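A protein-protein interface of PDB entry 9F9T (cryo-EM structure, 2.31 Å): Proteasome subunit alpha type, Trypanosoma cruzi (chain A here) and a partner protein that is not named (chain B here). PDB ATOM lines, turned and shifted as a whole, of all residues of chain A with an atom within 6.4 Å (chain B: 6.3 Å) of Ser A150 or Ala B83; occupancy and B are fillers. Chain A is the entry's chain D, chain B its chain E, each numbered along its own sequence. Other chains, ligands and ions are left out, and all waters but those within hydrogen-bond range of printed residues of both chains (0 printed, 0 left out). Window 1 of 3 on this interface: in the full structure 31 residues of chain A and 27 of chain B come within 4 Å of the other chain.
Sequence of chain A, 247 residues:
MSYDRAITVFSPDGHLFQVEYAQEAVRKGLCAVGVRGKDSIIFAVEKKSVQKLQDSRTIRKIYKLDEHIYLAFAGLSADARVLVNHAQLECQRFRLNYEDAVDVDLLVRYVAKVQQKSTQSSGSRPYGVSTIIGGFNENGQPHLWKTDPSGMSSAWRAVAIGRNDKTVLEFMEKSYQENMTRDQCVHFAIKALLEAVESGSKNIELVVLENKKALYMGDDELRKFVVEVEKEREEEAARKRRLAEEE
OD1 of Asp B84 sits at hydrogen-bond distance from NE2 of Gln A116, at 2.8 Å. The side-chain hydroxyl (OG) of Ser A153 lies within hydrogen-bond range of the guanidinium group (NH2) of Arg B86 (3.1 Å). The guanidinium group (NE) of Arg B135 lies within hydrogen-bond range of the backbone carbonyl oxygen (O) of Thr A119, 2.9 Å away.
O of Gln A116 is in hydrogen-bond range of OG1 of Thr A119, at 2.5 Å. The guanidinium group (NH1) of Arg B135 is in salt-bridge range of the side-chain carboxylate (OD2) of Asp B84. OG of Ser A150 lies within hydrogen-bond range of N of Met A152 (3.1 Å). The side-chain carboxylate (OD2) of Asp A148 sits at hydrogen-bond distance from the side-chain hydroxyl (OG) of Ser A150, at 2.6 Å.
Among the printed residues, merely in contact across the chains: Gln A116 with Ala B83 (3.6 Å), Gln A116 with Ile B87 (3.4 Å), Gln A116 with Arg B135 (3.9 Å), Ser A150 with Ala B83 (3.7 Å), Gly A151 with Ala B83 (3.7 Å), Gly A151 with Arg B86 (3.7 Å), Met A152 with Val B82 (3.6 Å), Met A152 with Ala B83 (3.9 Å) and Met A152 with Arg B86 (3.99 Å).
Ala A112 touches none of the printed residues of chain B. Printed residues of chain B within 4 Å of Gln A116: Ala B83, Asp B84, Ile B87 and Arg B135. Of the printed residues of chain B, Thr A119 touches Arg B135. Of chain B, only Ala B83 comes within 4 Å of Ser A150. Ala B83 touches just these residues of chain A: Gln A116, Ser A150, Gly A151 and Met A152. The nearest residue of chain B that does not touch Ser A150 is Asp B84 (5.2 Å). The nearest residue of chain A that does not touch Ala B83 is Ala A112 (5.8 Å). The nearest printed residue of chain A that does not touch Asp B84 is Thr A119 (4.6 Å).
Printed residues of chain B that touch a printed residue of chain A: Val B82, Ala B83, Asp B84, Arg B86, Ile B87 and Arg B135. Hydrophobic or aromatic side chains of chain B that line the printed part of chain A: Val B82, Ala B83 and Ile B87. Of the 12 printed residues of chain A, 6 touch a printed residue of chain B. Along chain A the printed residues that touch a printed residue of chain B span positions 116 to 153. Among the printed residues, 12 pairs touch across the chains.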
ATOM      1  N   VAL A  19     -20.354  19.298   1.444  1.00  0.00           N
ATOM      2  CA  VAL A  19     -21.033  19.402   2.745  1.00  0.00           C
ATOM      3  C   VAL A  19     -20.452  20.522   3.594  1.00  0.00           C
ATOM      4  O   VAL A  19     -21.223  21.224   4.229  1.00  0.00           O
ATOM      5  CB  VAL A  19     -21.093  18.083   3.554  1.00  0.00           C
ATOM      6  CG1 VAL A  19     -21.749  18.263   4.922  1.00  0.00           C
ATOM      7  CG2 VAL A  19     -21.814  16.988   2.765  1.00  0.00           C
ATOM      8  N   ALA A 112     -34.048  15.172   8.485  1.00  0.00           N
ATOM      9  CA  ALA A 112     -32.624  14.905   8.488  1.00  0.00           C
ATOM     10  C   ALA A 112     -32.237  13.923   7.389  1.00  0.00           C
ATOM     11  O   ALA A 112     -31.165  14.052   6.821  1.00  0.00           O
ATOM     12  CB  ALA A 112     -32.176  14.446   9.853  1.00  0.00           C
ATOM     13  N   GLN A 115     -31.969  15.675   4.157  1.00  0.00           N
ATOM     14  CA  GLN A 115     -30.701  16.360   3.998  1.00  0.00           C
ATOM     15  C   GLN A 115     -29.590  15.373   3.643  1.00  0.00           C
ATOM     16  O   GLN A 115     -28.726  15.703   2.836  1.00  0.00           O
ATOM     17  CB  GLN A 115     -30.380  17.238   5.221  1.00  0.00           C
ATOM     18  CG  GLN A 115     -31.527  18.183   5.633  1.00  0.00           C
ATOM     19  CD  GLN A 115     -31.090  19.340   6.495  1.00  0.00           C
ATOM     20  OE1 GLN A 115     -31.494  19.517   7.645  1.00  0.00           O
ATOM     21  NE2 GLN A 115     -30.229  20.157   5.906  1.00  0.00           N
ATOM     22  N   GLN A 116     -29.560  14.206   4.296  1.00  0.00           N
ATOM     23  CA  GLN A 116     -28.503  13.215   4.090  1.00  0.00           C
ATOM     24  C   GLN A 116     -28.517  12.726   2.641  1.00  0.00           C
ATOM     25  O   GLN A 116     -27.488  12.591   2.030  1.00  0.00           O
ATOM     26  CB  GLN A 116     -28.580  12.029   5.085  1.00  0.00           C
ATOM     27  CG  GLN A 116     -27.339  11.091   5.042  1.00  0.00           C
ATOM     28  CD  GLN A 116     -27.275  10.152   3.837  1.00  0.00           C
ATOM     29  OE1 GLN A 116     -28.288   9.730   3.262  1.00  0.00           O
ATOM     30  NE2 GLN A 116     -26.060   9.769   3.467  1.00  0.00           N
ATOM     31  N   LYS A 117     -29.686  12.576   2.068  1.00  0.00           N
ATOM     32  CA  LYS A 117     -29.786  11.984   0.749  1.00  0.00           C
ATOM     33  C   LYS A 117     -29.223  12.953  -0.258  1.00  0.00           C
ATOM     34  O   LYS A 117     -28.659  12.524  -1.252  1.00  0.00           O
ATOM     35  CB  LYS A 117     -31.237  11.599   0.437  1.00  0.00           C
ATOM     36  CG  LYS A 117     -31.754  10.390   1.228  1.00  0.00           C
ATOM     37  CD  LYS A 117     -33.209  10.018   0.929  1.00  0.00           C
ATOM     38  CE  LYS A 117     -33.495   8.552   1.196  1.00  0.00           C
ATOM     39  NZ  LYS A 117     -34.902   8.195   0.897  1.00  0.00           N
ATOM     40  N   THR A 119     -26.701  14.630   0.082  1.00  0.00           N
ATOM     41  CA  THR A 119     -25.242  14.541   0.113  1.00  0.00           C
ATOM     42  C   THR A 119     -24.735  13.313  -0.660  1.00  0.00           C
ATOM     43  O   THR A 119     -23.528  13.100  -0.798  1.00  0.00           O
ATOM     44  CB  THR A 119     -24.738  14.540   1.574  1.00  0.00           C
ATOM     45  OG1 THR A 119     -25.071  13.346   2.285  1.00  0.00           O
ATOM     46  CG2 THR A 119     -25.274  15.706   2.389  1.00  0.00           C
ATOM     47  N   ASP A 148     -28.380  19.558  10.612  1.00  0.00           N
ATOM     48  CA  ASP A 148     -27.339  20.280   9.910  1.00  0.00           C
ATOM     49  C   ASP A 148     -27.246  19.700   8.498  1.00  0.00           C
ATOM     50  O   ASP A 148     -27.934  18.734   8.207  1.00  0.00           O
ATOM     51  CB  ASP A 148     -26.060  20.312  10.755  1.00  0.00           C
ATOM     52  CG  ASP A 148     -25.224  19.035  10.755  1.00  0.00           C
ATOM     53  OD1 ASP A 148     -24.794  18.629  11.859  1.00  0.00           O
ATOM     54  OD2 ASP A 148     -24.950  18.474   9.654  1.00  0.00           O
ATOM     55  N   PRO A 149     -26.491  20.319   7.562  1.00  0.00           N
ATOM     56  CA  PRO A 149     -26.454  19.878   6.156  1.00  0.00           C
ATOM     57  C   PRO A 149     -26.009  18.445   5.843  1.00  0.00           C
ATOM     58  O   PRO A 149     -26.364  17.931   4.794  1.00  0.00           O
ATOM     59  CB  PRO A 149     -25.451  20.837   5.483  1.00  0.00           C
ATOM     60  CG  PRO A 149     -25.499  22.071   6.341  1.00  0.00           C
ATOM     61  CD  PRO A 149     -25.776  21.576   7.756  1.00  0.00           C
ATOM     62  N   SER A 150     -25.192  17.862   6.732  1.00  0.00           N
ATOM     63  CA  SER A 150     -24.729  16.490   6.608  1.00  0.00           C
ATOM     64  C   SER A 150     -25.896  15.525   6.757  1.00  0.00           C
ATOM     65  O   SER A 150     -25.877  14.450   6.131  1.00  0.00           O
ATOM     66  CB  SER A 150     -23.760  16.148   7.667  1.00  0.00           C
ATOM     67  OG  SER A 150     -24.470  16.040   8.894  1.00  0.00           O
ATOM     68  N   GLY A 151     -26.888  15.930   7.568  1.00  0.00           N
ATOM     69  CA  GLY A 151     -28.088  15.154   7.817  1.00  0.00           C
ATOM     70  C   GLY A 151     -28.161  14.676   9.270  1.00  0.00           C
ATOM     71  O   GLY A 151     -29.079  13.971   9.654  1.00  0.00           O
ATOM     72  N   MET A 152     -27.204  15.088  10.060  1.00  0.00           N
ATOM     73  CA  MET A 152     -27.089  14.726  11.451  1.00  0.00           C
ATOM     74  C   MET A 152     -28.091  15.526  12.287  1.00  0.00           C
ATOM     75  O   MET A 152     -28.130  16.736  12.179  1.00  0.00           O
ATOM     76  CB  MET A 152     -25.646  15.083  11.863  1.00  0.00           C
ATOM     77  CG  MET A 152     -25.351  14.870  13.315  1.00  0.00           C
ATOM     78  SD  MET A 152     -25.560  13.111  13.707  1.00  0.00           S
ATOM     79  CE  MET A 152     -25.613  13.182  15.499  1.00  0.00           C
ATOM     80  N   SER A 153     -28.914  14.862  13.094  1.00  0.00           N
ATOM     81  CA  SER A 153     -29.841  15.538  13.994  1.00  0.00           C
ATOM     82  C   SER A 153     -29.458  15.259  15.439  1.00  0.00           C
ATOM     83  O   SER A 153     -28.683  14.343  15.666  1.00  0.00           O
ATOM     84  CB  SER A 153     -31.289  15.155  13.732  1.00  0.00           C
ATOM     85  OG  SER A 153     -31.458  13.762  13.565  1.00  0.00           O
ATOM     86  N   GLY B  80     -17.714   6.980  12.360  1.00  0.00           N
ATOM     87  CA  GLY B  80     -17.666   7.759  11.139  1.00  0.00           C
ATOM     88  C   GLY B  80     -18.912   8.614  11.010  1.00  0.00           C
ATOM     89  O   GLY B  80     -19.442   9.152  11.969  1.00  0.00           O
ATOM     90  N   MET B  81     -19.387   8.778   9.806  1.00  0.00           N
ATOM     91  CA  MET B  81     -20.457   9.726   9.593  1.00  0.00           C
ATOM     92  C   MET B  81     -21.787   9.163  10.080  1.00  0.00           C
ATOM     93  O   MET B  81     -22.383   8.309   9.432  1.00  0.00           O
ATOM     94  CB  MET B  81     -20.521  10.027   8.097  1.00  0.00           C
ATOM     95  CG  MET B  81     -19.218  10.677   7.631  1.00  0.00           C
ATOM     96  SD  MET B  81     -19.306  11.109   5.902  1.00  0.00           S
ATOM     97  CE  MET B  81     -17.962  12.289   5.836  1.00  0.00           C
ATOM     98  N   VAL B  82     -22.279   9.714  11.184  1.00  0.00           N
ATOM     99  CA  VAL B  82     -23.486   9.204  11.813  1.00  0.00           C
ATOM    100  C   VAL B  82     -24.674   9.166  10.860  1.00  0.00           C
ATOM    101  O   VAL B  82     -25.418   8.197  10.857  1.00  0.00           O
ATOM    102  CB  VAL B  82     -23.834   9.980  13.087  1.00  0.00           C
ATOM    103  CG1 VAL B  82     -25.203   9.564  13.633  1.00  0.00           C
ATOM    104  CG2 VAL B  82     -22.758   9.769  14.139  1.00  0.00           C
ATOM    105  N   ALA B  83     -24.875  10.200  10.060  1.00  0.00           N
ATOM    106  CA  ALA B  83     -26.062  10.269   9.227  1.00  0.00           C
ATOM    107  C   ALA B  83     -26.066   9.181   8.150  1.00  0.00           C
ATOM    108  O   ALA B  83     -27.145   8.749   7.757  1.00  0.00           O
ATOM    109  CB  ALA B  83     -26.140  11.652   8.606  1.00  0.00           C
ATOM    110  N   ASP B  84     -24.892   8.820   7.629  1.00  0.00           N
ATOM    111  CA  ASP B  84     -24.725   7.729   6.671  1.00  0.00           C
ATOM    112  C   ASP B  84     -25.041   6.384   7.352  1.00  0.00           C
ATOM    113  O   ASP B  84     -25.672   5.527   6.767  1.00  0.00           O
ATOM    114  CB  ASP B  84     -23.301   7.724   6.086  1.00  0.00           C
ATOM    115  CG  ASP B  84     -22.940   8.847   5.101  1.00  0.00           C
ATOM    116  OD1 ASP B  84     -23.708   9.852   5.007  1.00  0.00           O
ATOM    117  OD2 ASP B  84     -21.910   8.715   4.395  1.00  0.00           O
ATOM    118  N   ALA B  85     -24.638   6.226   8.612  1.00  0.00           N
ATOM    119  CA  ALA B  85     -24.889   5.024   9.381  1.00  0.00           C
ATOM    120  C   ALA B  85     -26.377   4.799   9.569  1.00  0.00           C
ATOM    121  O   ALA B  85     -26.854   3.670   9.460  1.00  0.00           O
ATOM    122  CB  ALA B  85     -24.190   5.090  10.733  1.00  0.00           C
ATOM    123  N   ARG B  86     -27.121   5.862   9.832  1.00  0.00           N
ATOM    124  CA  ARG B  86     -28.573   5.768   9.866  1.00  0.00           C
ATOM    125  C   ARG B  86     -29.113   5.055   8.643  1.00  0.00           C
ATOM    126  O   ARG B  86     -30.001   4.239   8.775  1.00  0.00           O
ATOM    127  CB  ARG B  86     -29.203   7.132  10.113  1.00  0.00           C
ATOM    128  CG  ARG B  86     -28.841   7.659  11.499  1.00  0.00           C
ATOM    129  CD  ARG B  86     -29.842   8.666  12.012  1.00  0.00           C
ATOM    130  NE  ARG B  86     -29.358   9.372  13.197  1.00  0.00           N
ATOM    131  CZ  ARG B  86     -29.350  10.703  13.353  1.00  0.00           C
ATOM    132  NH1 ARG B  86     -28.992  11.236  14.514  1.00  0.00           N
ATOM    133  NH2 ARG B  86     -29.730  11.505  12.366  1.00  0.00           N
ATOM    134  N   ILE B  87     -28.562   5.281   7.466  1.00  0.00           N
ATOM    135  CA  ILE B  87     -29.089   4.619   6.273  1.00  0.00           C
ATOM    136  C   ILE B  87     -28.803   3.100   6.280  1.00  0.00           C
ATOM    137  O   ILE B  87     -29.676   2.320   5.943  1.00  0.00           O
ATOM    138  CB  ILE B  87     -28.509   5.299   5.021  1.00  0.00           C
ATOM    139  CG1 ILE B  87     -28.766   6.806   4.997  1.00  0.00           C
ATOM    140  CG2 ILE B  87     -28.970   4.617   3.754  1.00  0.00           C
ATOM    141  CD1 ILE B  87     -30.224   7.121   5.000  1.00  0.00           C
ATOM    142  N   LEU B  88     -27.561   2.684   6.590  1.00  0.00           N
ATOM    143  CA  LEU B  88     -27.213   1.278   6.734  1.00  0.00           C
ATOM    144  C   LEU B  88     -28.037   0.574   7.816  1.00  0.00           C
ATOM    145  O   LEU B  88     -28.373  -0.589   7.667  1.00  0.00           O
ATOM    146  CB  LEU B  88     -25.735   1.183   7.084  1.00  0.00           C
ATOM    147  CG  LEU B  88     -24.852   1.690   5.958  1.00  0.00           C
ATOM    148  CD1 LEU B  88     -23.414   1.385   6.239  1.00  0.00           C
ATOM    149  CD2 LEU B  88     -25.264   1.087   4.612  1.00  0.00           C
ATOM    150  N   ARG B 135     -21.062   8.330  -4.072  1.00  0.00           N
ATOM    151  CA  ARG B 135     -19.904   8.117  -3.235  1.00  0.00           C
ATOM    152  C   ARG B 135     -20.178   6.951  -2.304  1.00  0.00           C
ATOM    153  O   ARG B 135     -21.337   6.640  -2.015  1.00  0.00           O
ATOM    154  CB  ARG B 135     -19.611   9.376  -2.388  1.00  0.00           C
ATOM    155  CG  ARG B 135     -20.765   9.800  -1.485  1.00  0.00           C
ATOM    156  CD  ARG B 135     -20.406  11.000  -0.613  1.00  0.00           C
ATOM    157  NE  ARG B 135     -21.403  11.468   0.311  1.00  0.00           N
ATOM    158  CZ  ARG B 135     -21.666  10.877   1.470  1.00  0.00           C
ATOM    159  NH1 ARG B 135     -20.889   9.892   1.899  1.00  0.00           N
ATOM    160  NH2 ARG B 135     -22.674  11.307   2.220  1.00  0.00           N
ATOM    161  N   VAL B 139     -18.453   5.089   6.732  1.00  0.00           N
ATOM    162  CA  VAL B 139     -19.024   4.506   7.924  1.00  0.00           C
ATOM    163  C   VAL B 139     -18.444   3.132   8.136  1.00  0.00           C
ATOM    164  O   VAL B 139     -18.398   2.348   7.194  1.00  0.00           O
ATOM    165  CB  VAL B 139     -20.548   4.366   7.726  1.00  0.00           C
ATOM    166  CG1 VAL B 139     -21.209   3.441   8.745  1.00  0.00           C
ATOM    167  CG2 VAL B 139     -21.207   5.723   7.754  1.00  0.00           C
